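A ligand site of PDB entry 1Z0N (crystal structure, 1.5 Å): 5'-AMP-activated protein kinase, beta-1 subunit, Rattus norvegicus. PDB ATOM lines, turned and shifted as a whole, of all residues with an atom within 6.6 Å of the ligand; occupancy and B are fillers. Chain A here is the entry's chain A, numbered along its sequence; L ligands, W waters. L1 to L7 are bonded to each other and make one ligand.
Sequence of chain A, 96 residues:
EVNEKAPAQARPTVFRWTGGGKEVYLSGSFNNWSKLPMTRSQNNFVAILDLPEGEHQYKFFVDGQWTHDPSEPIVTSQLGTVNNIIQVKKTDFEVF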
ATOM      1  N   SER A  27      11.126  18.930  10.609  1.00  0.00           N
ATOM      2  CA  SER A  27      10.912  17.698  11.357  1.00  0.00           C
ATOM      3  C   SER A  27      12.206  17.323  12.066  1.00  0.00           C
ATOM      4  O   SER A  27      13.288  17.397  11.467  1.00  0.00           O
ATOM      5  CB  SER A  27      10.491  16.564  10.394  1.00  0.00           C
ATOM      6  OG  SER A  27      10.065  15.393  11.116  1.00  0.00           O
ATOM      7  N   ASN A  32       9.724  14.935  17.919  1.00  0.00           N
ATOM      8  CA  ASN A  32       9.359  13.534  17.714  1.00  0.00           C
ATOM      9  C   ASN A  32       8.995  13.282  16.231  1.00  0.00           C
ATOM     10  O   ASN A  32       8.129  12.465  15.891  1.00  0.00           O
ATOM     11  CB  ASN A  32       8.247  13.129  18.685  1.00  0.00           C
ATOM     12  CG  ASN A  32       8.617  13.405  20.097  1.00  0.00           C
ATOM     13  OD1 ASN A  32       9.681  13.012  20.553  1.00  0.00           O
ATOM     14  ND2 ASN A  32       7.783  14.191  20.783  1.00  0.00           N
ATOM     15  N   TRP A  33       9.745  13.956  15.352  1.00  0.00           N
ATOM     16  CA  TRP A  33       9.622  13.755  13.889  1.00  0.00           C
ATOM     17  C   TRP A  33       8.226  14.023  13.385  1.00  0.00           C
ATOM     18  O   TRP A  33       7.731  13.344  12.493  1.00  0.00           O
ATOM     19  CB  TRP A  33      10.153  12.379  13.471  1.00  0.00           C
ATOM     20  CG  TRP A  33      11.600  12.220  13.834  1.00  0.00           C
ATOM     21  CD1 TRP A  33      12.094  11.566  14.926  1.00  0.00           C
ATOM     22  CD2 TRP A  33      12.724  12.811  13.161  1.00  0.00           C
ATOM     23  NE1 TRP A  33      13.480  11.692  14.967  1.00  0.00           N
ATOM     24  CE2 TRP A  33      13.885  12.449  13.892  1.00  0.00           C
ATOM     25  CE3 TRP A  33      12.863  13.619  12.003  1.00  0.00           C
ATOM     26  CZ2 TRP A  33      15.184  12.872  13.515  1.00  0.00           C
ATOM     27  CZ3 TRP A  33      14.139  14.023  11.605  1.00  0.00           C
ATOM     28  CH2 TRP A  33      15.290  13.668  12.381  1.00  0.00           C
ATOM     29  N   LYS A  35       5.821  17.347  11.782  1.00  0.00           N
ATOM     30  CA  LYS A  35       6.104  18.279  10.714  1.00  0.00           C
ATOM     31  C   LYS A  35       5.604  19.659  11.080  1.00  0.00           C
ATOM     32  O   LYS A  35       4.392  19.922  11.061  1.00  0.00           O
ATOM     33  CB  LYS A  35       5.477  17.805   9.398  1.00  0.00           C
ATOM     34  CG  LYS A  35       6.168  16.536   8.798  1.00  0.00           C
ATOM     35  CD  LYS A  35       5.598  16.189   7.410  1.00  0.00           C
ATOM     36  CE  LYS A  35       6.177  14.891   6.884  1.00  0.00           C
ATOM     37  NZ  LYS A  35       5.752  13.716   7.684  1.00  0.00           N
ATOM     38  N   GLN A  57      18.922  16.292  15.849  1.00  0.00           N
ATOM     39  CA  GLN A  57      18.804  15.910  14.413  1.00  0.00           C
ATOM     40  C   GLN A  57      17.519  16.430  13.802  1.00  0.00           C
ATOM     41  O   GLN A  57      16.466  16.504  14.476  1.00  0.00           O
ATOM     42  CB  GLN A  57      18.837  14.385  14.274  1.00  0.00           C
ATOM     43  CG  GLN A  57      20.226  13.795  14.395  1.00  0.00           C
ATOM     44  CD  GLN A  57      20.202  12.276  14.469  1.00  0.00           C
ATOM     45  OE1 GLN A  57      19.671  11.604  13.574  1.00  0.00           O
ATOM     46  NE2 GLN A  57      20.746  11.725  15.547  1.00  0.00           N
ATOM     47  N   LYS A  59      15.432  17.444   9.674  1.00  0.00           N
ATOM     48  CA  LYS A  59      15.393  17.417   8.218  1.00  0.00           C
ATOM     49  C   LYS A  59      14.213  18.275   7.775  1.00  0.00           C
ATOM     50  O   LYS A  59      13.426  18.725   8.611  1.00  0.00           O
ATOM     51  CB  LYS A  59      15.195  15.949   7.729  1.00  0.00           C
ATOM     52  CG  LYS A  59      15.639  15.668   6.410  1.00  0.00           C
ATOM     53  CD  LYS A  59      15.624  14.186   6.172  1.00  0.00           C
ATOM     54  CE  LYS A  59      16.059  13.895   4.832  1.00  0.00           C
ATOM     55  NZ  LYS A  59      16.438  12.538   4.680  1.00  0.00           N
ATOM     56  N   TRP A  66      11.201  14.740   1.368  1.00  0.00           N
ATOM     57  CA  TRP A  66      12.216  14.805   2.433  1.00  0.00           C
ATOM     58  C   TRP A  66      13.565  15.261   1.866  1.00  0.00           C
ATOM     59  O   TRP A  66      14.033  14.724   0.853  1.00  0.00           O
ATOM     60  CB  TRP A  66      12.384  13.455   3.093  1.00  0.00           C
ATOM     61  CG  TRP A  66      11.234  13.063   3.969  1.00  0.00           C
ATOM     62  CD1 TRP A  66      10.193  12.227   3.639  1.00  0.00           C
ATOM     63  CD2 TRP A  66      11.014  13.454   5.313  1.00  0.00           C
ATOM     64  NE1 TRP A  66       9.356  12.071   4.715  1.00  0.00           N
ATOM     65  CE2 TRP A  66       9.842  12.812   5.760  1.00  0.00           C
ATOM     66  CE3 TRP A  66      11.714  14.284   6.204  1.00  0.00           C
ATOM     67  CZ2 TRP A  66       9.344  12.972   7.050  1.00  0.00           C
ATOM     68  CZ3 TRP A  66      11.240  14.415   7.497  1.00  0.00           C
ATOM     69  CH2 TRP A  66      10.048  13.784   7.904  1.00  0.00           C
ATOM     70  N   THR A  67      14.178  16.228   2.531  1.00  0.00           N
ATOM     71  CA  THR A  67      15.418  16.846   2.033  1.00  0.00           C
ATOM     72  C   THR A  67      16.220  17.346   3.197  1.00  0.00           C
ATOM     73  O   THR A  67      15.682  17.883   4.139  1.00  0.00           O
ATOM     74  CB  THR A  67      15.117  18.081   1.126  1.00  0.00           C
ATOM     75  OG1 THR A  67      13.992  17.791   0.261  1.00  0.00           O
ATOM     76  CG2 THR A  67      16.330  18.425   0.283  1.00  0.00           C
ATOM     77  N   SER A  77      21.026   8.175  10.214  1.00  0.00           N
ATOM     78  CA  SER A  77      20.248   7.688  11.346  1.00  0.00           C
ATOM     79  C   SER A  77      20.261   6.180  11.438  1.00  0.00           C
ATOM     80  O   SER A  77      20.659   5.476  10.496  1.00  0.00           O
ATOM     81  CB  SER A  77      18.803   8.144  11.233  1.00  0.00           C
ATOM     82  OG  SER A  77      18.147   7.424  10.206  1.00  0.00           O
ATOM     83  N   GLN A  78      19.684   5.685  12.514  1.00  0.00           N
ATOM     84  CA  GLN A  78      19.525   4.244  12.705  1.00  0.00           C
ATOM     85  C   GLN A  78      18.480   3.650  11.761  1.00  0.00           C
ATOM     86  O   GLN A  78      18.484   2.440  11.512  1.00  0.00           O
ATOM     87  CB  GLN A  78      19.191   3.941  14.163  1.00  0.00           C
ATOM     88  CG  GLN A  78      20.392   4.132  15.094  1.00  0.00           C
ATOM     89  CD  GLN A  78      21.519   3.192  14.762  1.00  0.00           C
ATOM     90  OE1 GLN A  78      21.426   1.991  15.029  1.00  0.00           O
ATOM     91  NE2 GLN A  78      22.585   3.715  14.178  1.00  0.00           N
ATOM     92  N   LEU A  79      17.630   4.490  11.198  1.00  0.00           N
ATOM     93  CA  LEU A  79      16.695   4.057  10.164  1.00  0.00           C
ATOM     94  C   LEU A  79      17.369   3.890   8.784  1.00  0.00           C
ATOM     95  O   LEU A  79      16.782   3.307   7.878  1.00  0.00           O
ATOM     96  CB  LEU A  79      15.502   5.016  10.069  1.00  0.00           C
ATOM     97  CG  LEU A  79      14.416   4.726   9.029  1.00  0.00           C
ATOM     98  CD1 LEU A  79      13.735   3.336   9.291  1.00  0.00           C
ATOM     99  CD2 LEU A  79      13.375   5.847   9.047  1.00  0.00           C
ATOM    100  N   GLY A  80      18.610   4.389   8.651  1.00  0.00           N
ATOM    101  CA  GLY A  80      19.299   4.379   7.362  1.00  0.00           C
ATOM    102  C   GLY A  80      18.884   5.556   6.499  1.00  0.00           C
ATOM    103  O   GLY A  80      18.643   5.406   5.293  1.00  0.00           O
ATOM    104  N   THR A  81      18.764   6.721   7.128  1.00  0.00           N
ATOM    105  CA  THR A  81      18.385   7.951   6.428  1.00  0.00           C
ATOM    106  C   THR A  81      19.325   9.060   6.816  1.00  0.00           C
ATOM    107  O   THR A  81      20.048   8.945   7.782  1.00  0.00           O
ATOM    108  CB  THR A  81      16.961   8.374   6.794  1.00  0.00           C
ATOM    109  OG1 THR A  81      16.875   8.638   8.196  1.00  0.00           O
ATOM    110  CG2 THR A  81      15.942   7.263   6.392  1.00  0.00           C
ATOM    111  N   VAL A  82      19.359  10.105   6.022  1.00  0.00           N
ATOM    112  CA  VAL A  82      20.301  11.210   6.282  1.00  0.00           C
ATOM    113  C   VAL A  82      19.597  12.373   6.978  1.00  0.00           C
ATOM    114  O   VAL A  82      18.619  12.913   6.464  1.00  0.00           O
ATOM    115  CB  VAL A  82      20.932  11.719   4.981  1.00  0.00           C
ATOM    116  CG1 VAL A  82      21.834  12.932   5.257  1.00  0.00           C
ATOM    117  CG2 VAL A  82      21.741  10.621   4.298  1.00  0.00           C
ATOM    118  N   ASN A  83      20.075  12.716   8.162  1.00  0.00           N
ATOM    119  CA  ASN A  83      19.594  13.888   8.885  1.00  0.00           C
ATOM    120  C   ASN A  83      20.656  14.958   8.982  1.00  0.00           C
ATOM    121  O   ASN A  83      21.843  14.650   9.079  1.00  0.00           O
ATOM    122  CB  ASN A  83      19.158  13.514  10.294  1.00  0.00           C
ATOM    123  CG  ASN A  83      17.976  12.604  10.295  1.00  0.00           C
ATOM    124  OD1 ASN A  83      17.163  12.661   9.393  1.00  0.00           O
ATOM    125  ND2 ASN A  83      17.893  11.714  11.323  1.00  0.00           N
HETATM  126  C1  LIG L   1      13.281   3.705   2.879  1.00  0.00           C
HETATM  127  C2  LIG L   1      14.151   4.762   2.262  1.00  0.00           C
HETATM  128  C3  LIG L   1      14.130   6.088   2.974  1.00  0.00           C
HETATM  129  C4  LIG L   1      12.770   6.516   3.483  1.00  0.00           C
HETATM  130  C5  LIG L   1      11.894   5.374   3.997  1.00  0.00           C
HETATM  131  C6  LIG L   1      10.441   5.765   4.195  1.00  0.00           C
HETATM  132  O1  LIG L   1      15.472   4.296   2.054  1.00  0.00           O
HETATM  133  O2  LIG L   1      14.739   7.089   2.217  1.00  0.00           O
HETATM  134  O3  LIG L   1      12.903   7.556   4.436  1.00  0.00           O
HETATM  135  O4  LIG L   1      12.011   4.143   3.295  1.00  0.00           O
HETATM  136  O5  LIG L   1       9.824   4.828   5.054  1.00  0.00           O
HETATM  137  C1  LG2 L   2      12.183   8.772   4.091  1.00  0.00           C
HETATM  138  C2  LG2 L   2      13.213   9.835   4.290  1.00  0.00           C
HETATM  139  C3  LG2 L   2      13.605  10.040   5.739  1.00  0.00           C
HETATM  140  C4  LG2 L   2      12.482   9.962   6.770  1.00  0.00           C
HETATM  141  C5  LG2 L   2      11.389   8.964   6.409  1.00  0.00           C
HETATM  142  C6  LG2 L   2      10.098   9.142   7.185  1.00  0.00           C
HETATM  143  O1  LG2 L   2      14.341   9.623   3.430  1.00  0.00           O
HETATM  144  O2  LG2 L   2      14.449  11.133   5.945  1.00  0.00           O
HETATM  145  O3  LG2 L   2      12.997   9.699   8.070  1.00  0.00           O
HETATM  146  O4  LG2 L   2      11.116   8.812   5.036  1.00  0.00           O
HETATM  147  O5  LG2 L   2       9.303   7.973   6.935  1.00  0.00           O
HETATM  148  C1  LG3 L   3      15.366  -0.181   5.941  1.00  0.00           C
HETATM  149  C2  LG3 L   3      16.382   0.650   5.177  1.00  0.00           C
HETATM  150  C3  LG3 L   3      15.875   1.959   4.586  1.00  0.00           C
HETATM  151  C4  LG3 L   3      14.420   2.001   4.155  1.00  0.00           C
HETATM  152  C5  LG3 L   3      13.462   1.064   4.879  1.00  0.00           C
HETATM  153  C6  LG3 L   3      12.282   0.682   3.987  1.00  0.00           C
HETATM  154  O1  LG3 L   3      17.577   0.818   5.958  1.00  0.00           O
HETATM  155  O2  LG3 L   3      16.683   2.404   3.527  1.00  0.00           O
HETATM  156  O3  LG3 L   3      13.938   3.343   4.118  1.00  0.00           O
HETATM  157  O4  LG3 L   3      14.014  -0.133   5.478  1.00  0.00           O
HETATM  158  O5  LG3 L   3      11.163   1.387   4.421  1.00  0.00           O
HETATM  159  C1  LG4 L   4      12.958  10.813   8.980  1.00  0.00           C
HETATM  160  C2  LG4 L   4      14.331  10.817   9.607  1.00  0.00           C
HETATM  161  C3  LG4 L   4      14.606   9.696  10.608  1.00  0.00           C
HETATM  162  C4  LG4 L   4      13.495   9.382  11.562  1.00  0.00           C
HETATM  163  C5  LG4 L   4      12.134   9.452  10.874  1.00  0.00           C
HETATM  164  C6  LG4 L   4      10.918   9.096  11.752  1.00  0.00           C
HETATM  165  O1  LG4 L   4      15.313  10.927   8.607  1.00  0.00           O
HETATM  166  O2  LG4 L   4      15.870   9.745  11.241  1.00  0.00           O
HETATM  167  O3  LG4 L   4      13.730   8.165  12.250  1.00  0.00           O
HETATM  168  O4  LG4 L   4      11.909  10.493   9.907  1.00  0.00           O
HETATM  169  O5  LG4 L   4       9.761   8.903  10.909  1.00  0.00           O
HETATM  170  C1  LG5 L   5      15.272  -0.758  11.190  1.00  0.00           C
HETATM  171  C2  LG5 L   5      16.600  -0.837  10.479  1.00  0.00           C
HETATM  172  C3  LG5 L   5      16.615  -0.283   9.095  1.00  0.00           C
HETATM  173  C4  LG5 L   5      15.385  -0.541   8.263  1.00  0.00           C
HETATM  174  C5  LG5 L   5      14.072  -0.615   9.036  1.00  0.00           C
HETATM  175  C6  LG5 L   5      12.986  -1.392   8.301  1.00  0.00           C
HETATM  176  O1  LG5 L   5      17.662  -0.334  11.261  1.00  0.00           O
HETATM  177  O2  LG5 L   5      17.825  -0.519   8.403  1.00  0.00           O
HETATM  178  O3  LG5 L   5      15.300   0.401   7.220  1.00  0.00           O
HETATM  179  O4  LG5 L   5      14.147  -1.062  10.388  1.00  0.00           O
HETATM  180  O5  LG5 L   5      11.718  -0.968   8.794  1.00  0.00           O
HETATM  181  C1  LG6 L   6      13.669   8.259  13.670  1.00  0.00           C
HETATM  182  C2  LG6 L   6      14.980   7.745  14.186  1.00  0.00           C
HETATM  183  C3  LG6 L   6      15.188   6.269  14.039  1.00  0.00           C
HETATM  184  C4  LG6 L   6      13.961   5.422  14.332  1.00  0.00           C
HETATM  185  C5  LG6 L   6      12.627   6.030  13.923  1.00  0.00           C
HETATM  186  C6  LG6 L   6      11.436   5.375  14.613  1.00  0.00           C
HETATM  187  O1  LG6 L   6      16.057   8.459  13.602  1.00  0.00           O
HETATM  188  O2  LG6 L   6      16.314   5.817  14.734  1.00  0.00           O
HETATM  189  O3  LG6 L   6      14.136   4.147  13.764  1.00  0.00           O
HETATM  190  O4  LG6 L   6      12.514   7.464  14.001  1.00  0.00           O
HETATM  191  O5  LG6 L   6      10.296   5.680  13.841  1.00  0.00           O
HETATM  192  C1  LG7 L   7      13.898   3.044  14.698  1.00  0.00           C
HETATM  193  C2  LG7 L   7      15.249   2.339  14.867  1.00  0.00           C
HETATM  194  C3  LG7 L   7      15.745   1.574  13.662  1.00  0.00           C
HETATM  195  C4  LG7 L   7      14.663   0.861  12.858  1.00  0.00           C
HETATM  196  C5  LG7 L   7      13.264   1.503  12.877  1.00  0.00           C
HETATM  197  C6  LG7 L   7      12.142   0.511  12.584  1.00  0.00           C
HETATM  198  O1  LG7 L   7      16.253   3.179  15.464  1.00  0.00           O
HETATM  199  O2  LG7 L   7      16.860   0.730  13.963  1.00  0.00           O
HETATM  200  O3  LG7 L   7      15.102   0.650  11.529  1.00  0.00           O
HETATM  201  O4  LG7 L   7      12.903   2.298  14.026  1.00  0.00           O
HETATM  202  O5  LG7 L   7      11.084   1.235  11.944  1.00  0.00           O
HETATM  203  O   HOH W   1      20.073   1.112   8.844  1.00  0.00           O
HETATM  204  O   HOH W   2      18.087   9.818  14.836  1.00  0.00           O
HETATM  205  O   HOH W   3      18.068   2.027  17.172  1.00  0.00           O
HETATM  206  O   HOH W   4      18.649  -2.699  12.365  1.00  0.00           O
HETATM  207  O   HOH W   5      19.142   2.951   3.988  1.00  0.00           O
HETATM  208  O   HOH W   6      13.412   7.376  -0.130  1.00  0.00           O
HETATM  209  O   HOH W   7       6.802   9.434   8.315  1.00  0.00           O
HETATM  210  O   HOH W   8       9.494   6.352   9.579  1.00  0.00           O
HETATM  211  O   HOH W   9       8.117  10.985  10.963  1.00  0.00           O
HETATM  212  O   HOH W  10      16.130   3.426  -0.282  1.00  0.00           O
HETATM  213  O   HOH W  11      17.331   6.789  16.865  1.00  0.00           O
HETATM  214  O   HOH W  12      17.403  10.128   3.927  1.00  0.00           O
HETATM  215  O   HOH W  13      14.050  10.835   1.055  1.00  0.00           O
HETATM  216  O   HOH W  14      19.250   7.336  14.871  1.00  0.00           O
HETATM  217  O   HOH W  15       8.123   8.293   4.296  1.00  0.00           O
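O of Gln 78 sits at hydrogen-bond distance from O1 of LG5 L5. The side-chain hydroxyl (OG) of Ser 77 sits close to an oxygen (O2) of LG4 L4, at 3.4 Å. The side-chain amide oxygen (OD1) of Asn 83 sits at hydrogen-bond distance from an oxygen (O1) of LG4 L4 (2.7 Å). O1 of LG4 L4 lies within hydrogen-bond range of OG1 of Thr 81, 2.8 Å away. The backbone carbonyl oxygen (O) of Leu 79 sits at hydrogen-bond distance from an oxygen (O1) of LG3 L3 (3.2 Å). The side-chain amino group (NZ) of Lys 59 lies within hydrogen-bond range of an oxygen (O2) of LG2 L2, 2.7 Å away.
The side-chain amide nitrogen (ND2) of Asn 83 lies within hydrogen-bond range of the side-chain amide oxygen (OE1) of Gln 57, 2.9 Å away. OG of Ser 77 sits at hydrogen-bond distance from OG1 of Thr 81, 2.7 Å away. OG of Ser 77 lies close to N of Leu 79, 3.1 Å away. The backbone NH (N) of Lys 59 lies within hydrogen-bond range of the backbone carbonyl oxygen (O) of Ser 27 (2.8 Å). The side-chain hydroxyl (OG) of Ser 77 lies within hydrogen-bond range of the backbone NH (N) of Gly 80, at 3.4 Å. The side-chain hydroxyl (OG) of Ser 27 sits close to the backbone carbonyl oxygen (O) of Trp 33 (3.4 Å). The side-chain amino group (NZ) of Lys 59 is in hydrogen-bond range of the backbone carbonyl oxygen (O) of Val 82 (2.8 Å).
Water W5 lies within hydrogen-bond range of an oxygen (O2) of LG3 L3 and the backbone carbonyl oxygen (O) of Gly 80. Water W9 bridges O5 of LG4 L4 and O of Trp 33. Water W2 bridges OE1 of Gln 57 (2.7 Å) and O1 of LG6 L6 (2.7 Å). Water W1 lies within hydrogen-bond range of O2 of LG5 L5 (2.8 Å) and O of Gln 78 (3.4 Å). Water W12 lies within hydrogen-bond range of NZ of Lys 59, N of Val 82 and O1 of LG2 L2. Water W14 bridges the backbone NH (N) of Gln 78 (2.9 Å) and an oxygen (O2) of LG6 L6 (3.3 Å).
Residues that only touch the ligand: Trp 33, Trp 66 and Gly 80. Hydrophobic or aromatic side chains that line the ligand: Trp 33, Trp 66 and Leu 79. Of the 15 residues printed, 9 come within 4 Å of the ligand. The nearest printed residue that does not touch the ligand is Val 82 (4.4 Å).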
